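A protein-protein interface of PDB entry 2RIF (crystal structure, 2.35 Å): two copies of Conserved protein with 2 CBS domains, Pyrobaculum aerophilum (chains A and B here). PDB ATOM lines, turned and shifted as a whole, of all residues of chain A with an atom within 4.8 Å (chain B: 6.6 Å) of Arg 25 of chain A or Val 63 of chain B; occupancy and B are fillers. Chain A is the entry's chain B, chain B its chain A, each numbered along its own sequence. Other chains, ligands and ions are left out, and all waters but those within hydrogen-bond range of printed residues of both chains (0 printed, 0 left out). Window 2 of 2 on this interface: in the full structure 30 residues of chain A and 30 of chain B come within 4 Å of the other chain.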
ATOM      1  N   THR A  23     -26.675  26.323   2.506  1.00  0.00           N
ATOM      2  CA  THR A  23     -27.427  25.307   3.241  1.00  0.00           C
ATOM      3  C   THR A  23     -27.753  25.823   4.639  1.00  0.00           C
ATOM      4  O   THR A  23     -27.209  26.841   5.076  1.00  0.00           O
ATOM      5  CB  THR A  23     -26.645  23.979   3.360  1.00  0.00           C
ATOM      6  OG1 THR A  23     -25.531  24.144   4.247  1.00  0.00           O
ATOM      7  CG2 THR A  23     -26.148  23.514   1.992  1.00  0.00           C
ATOM      8  N   ILE A  24     -28.635  25.115   5.337  1.00  0.00           N
ATOM      9  CA  ILE A  24     -29.052  25.513   6.682  1.00  0.00           C
ATOM     10  C   ILE A  24     -27.870  25.513   7.654  1.00  0.00           C
ATOM     11  O   ILE A  24     -27.719  26.446   8.446  1.00  0.00           O
ATOM     12  CB  ILE A  24     -30.180  24.601   7.223  1.00  0.00           C
ATOM     13  CG1 ILE A  24     -31.466  24.804   6.417  1.00  0.00           C
ATOM     14  CG2 ILE A  24     -30.453  24.894   8.694  1.00  0.00           C
ATOM     15  CD1 ILE A  24     -32.562  23.808   6.747  1.00  0.00           C
ATOM     16  N   ARG A  25     -27.034  24.478   7.581  1.00  0.00           N
ATOM     17  CA  ARG A  25     -25.855  24.375   8.449  1.00  0.00           C
ATOM     18  C   ARG A  25     -24.812  25.440   8.110  1.00  0.00           C
ATOM     19  O   ARG A  25     -24.183  25.996   9.011  1.00  0.00           O
ATOM     20  CB  ARG A  25     -25.220  22.983   8.363  1.00  0.00           C
ATOM     21  CG  ARG A  25     -24.242  22.687   9.496  1.00  0.00           C
ATOM     22  CD  ARG A  25     -23.586  21.318   9.356  1.00  0.00           C
ATOM     23  NE  ARG A  25     -24.552  20.217   9.313  1.00  0.00           N
ATOM     24  CZ  ARG A  25     -25.202  19.727  10.369  1.00  0.00           C
ATOM     25  NH1 ARG A  25     -25.014  20.227  11.586  1.00  0.00           N
ATOM     26  NH2 ARG A  25     -26.056  18.722  10.206  1.00  0.00           N
ATOM     27  N   GLU A  26     -24.629  25.712   6.818  1.00  0.00           N
ATOM     28  CA  GLU A  26     -23.692  26.749   6.367  1.00  0.00           C
ATOM     29  C   GLU A  26     -24.046  28.116   6.950  1.00  0.00           C
ATOM     30  O   GLU A  26     -23.157  28.882   7.324  1.00  0.00           O
ATOM     31  CB  GLU A  26     -23.642  26.820   4.835  1.00  0.00           C
ATOM     32  CG  GLU A  26     -22.800  25.717   4.200  1.00  0.00           C
ATOM     33  CD  GLU A  26     -22.926  25.657   2.683  1.00  0.00           C
ATOM     34  OE1 GLU A  26     -23.558  26.556   2.088  1.00  0.00           O
ATOM     35  OE2 GLU A  26     -22.386  24.704   2.084  1.00  0.00           O
ATOM     36  N   VAL A  27     -25.343  28.409   7.031  1.00  0.00           N
ATOM     37  CA  VAL A  27     -25.824  29.629   7.682  1.00  0.00           C
ATOM     38  C   VAL A  27     -25.542  29.569   9.183  1.00  0.00           C
ATOM     39  O   VAL A  27     -25.096  30.549   9.772  1.00  0.00           O
ATOM     40  CB  VAL A  27     -27.338  29.833   7.456  1.00  0.00           C
ATOM     41  CG1 VAL A  27     -27.854  31.009   8.272  1.00  0.00           C
ATOM     42  CG2 VAL A  27     -27.627  30.040   5.979  1.00  0.00           C
ATOM     43  N   ALA A  28     -25.798  28.408   9.785  1.00  0.00           N
ATOM     44  CA  ALA A  28     -25.557  28.186  11.213  1.00  0.00           C
ATOM     45  C   ALA A  28     -24.095  28.422  11.583  1.00  0.00           C
ATOM     46  O   ALA A  28     -23.801  29.045  12.604  1.00  0.00           O
ATOM     47  CB  ALA A  28     -25.971  26.774  11.601  1.00  0.00           C
ATOM     48  N   THR A  29     -23.189  27.919  10.747  1.00  0.00           N
ATOM     49  CA  THR A  29     -21.752  28.109  10.945  1.00  0.00           C
ATOM     50  C   THR A  29     -21.379  29.585  10.862  1.00  0.00           C
ATOM     51  O   THR A  29     -20.605  30.085  11.681  1.00  0.00           O
ATOM     52  CB  THR A  29     -20.928  27.347   9.885  1.00  0.00           C
ATOM     53  OG1 THR A  29     -21.302  25.965   9.878  1.00  0.00           O
ATOM     54  CG2 THR A  29     -19.437  27.466  10.170  1.00  0.00           C
ATOM     55  N   ILE A  59     -33.520  28.614  12.270  1.00  0.00           N
ATOM     56  CA  ILE A  59     -32.712  27.405  12.414  1.00  0.00           C
ATOM     57  C   ILE A  59     -33.186  26.561  13.600  1.00  0.00           C
ATOM     58  O   ILE A  59     -33.169  25.333  13.533  1.00  0.00           O
ATOM     59  CB  ILE A  59     -31.206  27.747  12.555  1.00  0.00           C
ATOM     60  CG1 ILE A  59     -30.677  28.308  11.231  1.00  0.00           C
ATOM     61  CG2 ILE A  59     -30.398  26.518  12.954  1.00  0.00           C
ATOM     62  CD1 ILE A  59     -29.209  28.690  11.266  1.00  0.00           C
ATOM     63  N   VAL A  63     -34.481  22.697  13.564  1.00  0.00           N
ATOM     64  CA  VAL A  63     -33.972  21.668  14.475  1.00  0.00           C
ATOM     65  C   VAL A  63     -35.112  20.920  15.170  1.00  0.00           C
ATOM     66  O   VAL A  63     -35.072  19.693  15.286  1.00  0.00           O
ATOM     67  CB  VAL A  63     -33.035  22.279  15.548  1.00  0.00           C
ATOM     68  CG1 VAL A  63     -32.697  21.254  16.623  1.00  0.00           C
ATOM     69  CG2 VAL A  63     -31.766  22.814  14.902  1.00  0.00           C
ATOM     70  N   LEU A  69     -30.507  19.381   7.932  1.00  0.00           N
ATOM     71  CA  LEU A  69     -29.713  20.577   8.212  1.00  0.00           C
ATOM     72  C   LEU A  69     -28.658  20.862   7.139  1.00  0.00           C
ATOM     73  O   LEU A  69     -28.023  21.918   7.162  1.00  0.00           O
ATOM     74  CB  LEU A  69     -29.059  20.470   9.594  1.00  0.00           C
ATOM     75  CG  LEU A  69     -30.039  20.316  10.763  1.00  0.00           C
ATOM     76  CD1 LEU A  69     -29.289  20.113  12.068  1.00  0.00           C
ATOM     77  CD2 LEU A  69     -30.979  21.515  10.859  1.00  0.00           C
ATOM     78  N   ASP A  70     -28.470  19.922   6.212  1.00  0.00           N
ATOM     79  CA  ASP A  70     -27.619  20.132   5.040  1.00  0.00           C
ATOM     80  C   ASP A  70     -28.446  20.442   3.787  1.00  0.00           C
ATOM     81  O   ASP A  70     -27.898  20.542   2.687  1.00  0.00           O
ATOM     82  CB  ASP A  70     -26.727  18.911   4.805  1.00  0.00           C
ATOM     83  CG  ASP A  70     -25.663  18.756   5.872  1.00  0.00           C
ATOM     84  OD1 ASP A  70     -24.978  19.756   6.176  1.00  0.00           O
ATOM     85  OD2 ASP A  70     -25.502  17.636   6.399  1.00  0.00           O
ATOM     86  N   ASP B  58     -27.552  29.037  21.758  1.00  0.00           N
ATOM     87  CA  ASP B  58     -26.728  27.905  22.203  1.00  0.00           C
ATOM     88  C   ASP B  58     -26.996  26.684  21.329  1.00  0.00           C
ATOM     89  O   ASP B  58     -26.074  25.957  20.968  1.00  0.00           O
ATOM     90  CB  ASP B  58     -27.005  27.556  23.669  1.00  0.00           C
ATOM     91  CG  ASP B  58     -26.784  28.729  24.605  1.00  0.00           C
ATOM     92  OD1 ASP B  58     -25.706  29.358  24.544  1.00  0.00           O
ATOM     93  OD2 ASP B  58     -27.689  29.016  25.411  1.00  0.00           O
ATOM     94  N   ILE B  59     -28.263  26.470  20.990  1.00  0.00           N
ATOM     95  CA  ILE B  59     -28.653  25.387  20.090  1.00  0.00           C
ATOM     96  C   ILE B  59     -28.042  25.602  18.701  1.00  0.00           C
ATOM     97  O   ILE B  59     -27.597  24.648  18.062  1.00  0.00           O
ATOM     98  CB  ILE B  59     -30.192  25.266  19.991  1.00  0.00           C
ATOM     99  CG1 ILE B  59     -30.769  24.797  21.332  1.00  0.00           C
ATOM    100  CG2 ILE B  59     -30.595  24.297  18.886  1.00  0.00           C
ATOM    101  CD1 ILE B  59     -32.283  24.784  21.373  1.00  0.00           C
ATOM    102  N   LEU B  60     -28.007  26.858  18.253  1.00  0.00           N
ATOM    103  CA  LEU B  60     -27.406  27.216  16.964  1.00  0.00           C
ATOM    104  C   LEU B  60     -25.938  26.789  16.884  1.00  0.00           C
ATOM    105  O   LEU B  60     -25.500  26.263  15.862  1.00  0.00           O
ATOM    106  CB  LEU B  60     -27.519  28.725  16.721  1.00  0.00           C
ATOM    107  CG  LEU B  60     -26.981  29.271  15.394  1.00  0.00           C
ATOM    108  CD1 LEU B  60     -27.890  28.872  14.250  1.00  0.00           C
ATOM    109  CD2 LEU B  60     -26.839  30.787  15.464  1.00  0.00           C
ATOM    110  N   ARG B  61     -25.186  27.022  17.957  1.00  0.00           N
ATOM    111  CA  ARG B  61     -23.781  26.608  18.014  1.00  0.00           C
ATOM    112  C   ARG B  61     -23.655  25.087  18.020  1.00  0.00           C
ATOM    113  O   ARG B  61     -22.741  24.533  17.409  1.00  0.00           O
ATOM    114  CB  ARG B  61     -23.083  27.186  19.243  1.00  0.00           C
ATOM    115  CG  ARG B  61     -23.035  28.699  19.265  1.00  0.00           C
ATOM    116  CD  ARG B  61     -21.950  29.199  20.194  1.00  0.00           C
ATOM    117  NE  ARG B  61     -22.151  30.594  20.590  1.00  0.00           N
ATOM    118  CZ  ARG B  61     -22.769  30.997  21.702  1.00  0.00           C
ATOM    119  NH1 ARG B  61     -22.888  32.297  21.952  1.00  0.00           N
ATOM    120  NH2 ARG B  61     -23.274  30.118  22.568  1.00  0.00           N
ATOM    121  N   ALA B  62     -24.574  24.424  18.720  1.00  0.00           N
ATOM    122  CA  ALA B  62     -24.643  22.965  18.730  1.00  0.00           C
ATOM    123  C   ALA B  62     -24.807  22.428  17.310  1.00  0.00           C
ATOM    124  O   ALA B  62     -24.165  21.447  16.935  1.00  0.00           O
ATOM    125  CB  ALA B  62     -25.788  22.488  19.614  1.00  0.00           C
ATOM    126  N   VAL B  63     -25.660  23.083  16.524  1.00  0.00           N
ATOM    127  CA  VAL B  63     -25.848  22.724  15.121  1.00  0.00           C
ATOM    128  C   VAL B  63     -24.560  22.957  14.331  1.00  0.00           C
ATOM    129  O   VAL B  63     -24.095  22.066  13.625  1.00  0.00           O
ATOM    130  CB  VAL B  63     -26.996  23.528  14.465  1.00  0.00           C
ATOM    131  CG1 VAL B  63     -27.094  23.207  12.980  1.00  0.00           C
ATOM    132  CG2 VAL B  63     -28.319  23.242  15.160  1.00  0.00           C
ATOM    133  N   ALA B  64     -23.983  24.148  14.467  1.00  0.00           N
ATOM    134  CA  ALA B  64     -22.765  24.512  13.736  1.00  0.00           C
ATOM    135  C   ALA B  64     -21.572  23.607  14.069  1.00  0.00           C
ATOM    136  O   ALA B  64     -20.777  23.278  13.187  1.00  0.00           O
ATOM    137  CB  ALA B  64     -22.409  25.970  14.002  1.00  0.00           C
ATOM    138  N   GLN B  65     -21.457  23.208  15.334  1.00  0.00           N
ATOM    139  CA  GLN B  65     -20.368  22.332  15.784  1.00  0.00           C
ATOM    140  C   GLN B  65     -20.689  20.841  15.616  1.00  0.00           C
ATOM    141  O   GLN B  65     -19.900  19.987  16.021  1.00  0.00           O
ATOM    142  CB  GLN B  65     -20.020  22.626  17.245  1.00  0.00           C
ATOM    143  CG  GLN B  65     -19.404  23.993  17.471  1.00  0.00           C
ATOM    144  CD  GLN B  65     -19.245  24.317  18.942  1.00  0.00           C
ATOM    145  OE1 GLN B  65     -19.771  25.319  19.427  1.00  0.00           O
ATOM    146  NE2 GLN B  65     -18.532  23.460  19.667  1.00  0.00           N
ATOM    147  N   ARG B  66     -21.848  20.540  15.030  1.00  0.00           N
ATOM    148  CA  ARG B  66     -22.263  19.167  14.727  1.00  0.00           C
ATOM    149  C   ARG B  66     -22.285  18.274  15.966  1.00  0.00           C
ATOM    150  O   ARG B  66     -21.884  17.111  15.917  1.00  0.00           O
ATOM    151  CB  ARG B  66     -21.370  18.570  13.633  1.00  0.00           C
ATOM    152  CG  ARG B  66     -21.176  19.508  12.454  1.00  0.00           C
ATOM    153  CD  ARG B  66     -20.676  18.810  11.203  1.00  0.00           C
ATOM    154  NE  ARG B  66     -21.727  18.013  10.567  1.00  0.00           N
ATOM    155  CZ  ARG B  66     -21.872  17.836   9.252  1.00  0.00           C
ATOM    156  NH1 ARG B  66     -21.050  18.414   8.379  1.00  0.00           N
ATOM    157  NH2 ARG B  66     -22.871  17.084   8.800  1.00  0.00           N
ATOM    158  N   LEU B  67     -22.769  18.829  17.074  1.00  0.00           N
ATOM    159  CA  LEU B  67     -22.911  18.076  18.311  1.00  0.00           C
ATOM    160  C   LEU B  67     -24.088  17.118  18.186  1.00  0.00           C
ATOM    161  O   LEU B  67     -24.957  17.295  17.329  1.00  0.00           O
ATOM    162  CB  LEU B  67     -23.149  19.018  19.496  1.00  0.00           C
ATOM    163  CG  LEU B  67     -22.096  20.096  19.768  1.00  0.00           C
ATOM    164  CD1 LEU B  67     -22.520  20.960  20.947  1.00  0.00           C
ATOM    165  CD2 LEU B  67     -20.729  19.476  20.015  1.00  0.00           C
ATOM    166  N   LEU B  69     -27.423  16.253  19.024  1.00  0.00           N
ATOM    167  CA  LEU B  69     -28.566  17.007  19.551  1.00  0.00           C
ATOM    168  C   LEU B  69     -29.424  16.197  20.534  1.00  0.00           C
ATOM    169  O   LEU B  69     -30.296  16.756  21.203  1.00  0.00           O
ATOM    170  CB  LEU B  69     -29.434  17.561  18.411  1.00  0.00           C
ATOM    171  CG  LEU B  69     -28.841  18.732  17.617  1.00  0.00           C
ATOM    172  CD1 LEU B  69     -27.839  18.266  16.575  1.00  0.00           C
ATOM    173  CD2 LEU B  69     -29.943  19.535  16.955  1.00  0.00           C
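Among the printed residues, merely in contact across the chains: Arg 25 of chain A with Arg 66 of chain B, Ala 28 of chain A with Leu 60 of chain B, Ala 28 of chain A with Val 63 of chain B, Ala 28 of chain A with Ala 64 of chain B, Thr 29 of chain A with Ala 64 of chain B, Ile 59 of chain A with Leu 60 of chain B, Val 63 of chain A with Val 63 of chain B, Val 63 of chain A with Leu 69 of chain B and Leu 69 of chain A with Val 63 of chain B.
Of the 11 printed residues of chain B, 5 touch a printed residue of chain A.
Hydrophobic or aromatic side chains of chain B that line the printed part of chain A: Leu 60, Val 63, Ala 64 and Leu 69.
Along chain B the printed residues that touch a printed residue of chain A span positions 60 to 69.
Hydrophobic or aromatic side chains of chain A within 4 Å of the printed part of chain B: Ala 28, Ile 59, Val 63 and Leu 69.
OG1 of Thr 29 of chain A sits at hydrogen-bond distance from O of Arg 25 of chain A (3.0 Å).
The backbone NH (N) of Arg 25 of chain A is in hydrogen-bond range of the backbone carbonyl oxygen (O) of Leu 69 of chain A (2.8 Å).
The side-chain carboxylate (OD1) of Asp 70 of chain A is in salt-bridge range of the guanidinium group (NE) of Arg 25 of chain A (3.2 Å).
Arg 25 of chain A touches two residues of chain B.
Val 27 of chain A touches none of the printed residues of chain B.
Of the printed residues of chain B, Ala 28 of chain A touches Leu 60, Val 63 and Ala 64.
Of the printed residues of chain B, Leu 69 of chain A touches Val 63 (3.9 Å).
Of the printed residues of chain A, Val 63 of chain B touches Arg 25 (2.9 Å), Ala 28 (3.99 Å), Val 63 (3.5 Å) and Leu 69 (3.9 Å).
The nearest residue of chain B that does not touch Arg 25 of chain A is Ala 64 of chain B (4.8 Å).
The nearest printed residue of chain A that does not touch Val 63 of chain B is Ile 59 of chain A (4.5 Å).
The nearest printed residue of chain B that does not touch Leu 69 of chain A is Leu 69 of chain B (5.0 Å).
The backbone carbonyl oxygen (O) of Val 63 of chain B lies within hydrogen-bond range of the guanidinium group (NH1) of Arg 25 of chain A, at 2.9 Å.
The guanidinium group (NH2) of Arg 66 of chain B lies within salt-bridge range of the side-chain carboxylate (OD2) of Asp 70 of chain A (3.6 Å).
Val 63 of chain A touches its own counterpart, Val 63 of chain B.
Val 63 of chain A touches Leu 69 of chain B, and with the chains exchanged Leu 69 of chain A touches Val 63 of chain B.
Of the 11 pairs that touch across the chains among the printed residues, 3 have their exchanged pair printed and touching as well.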
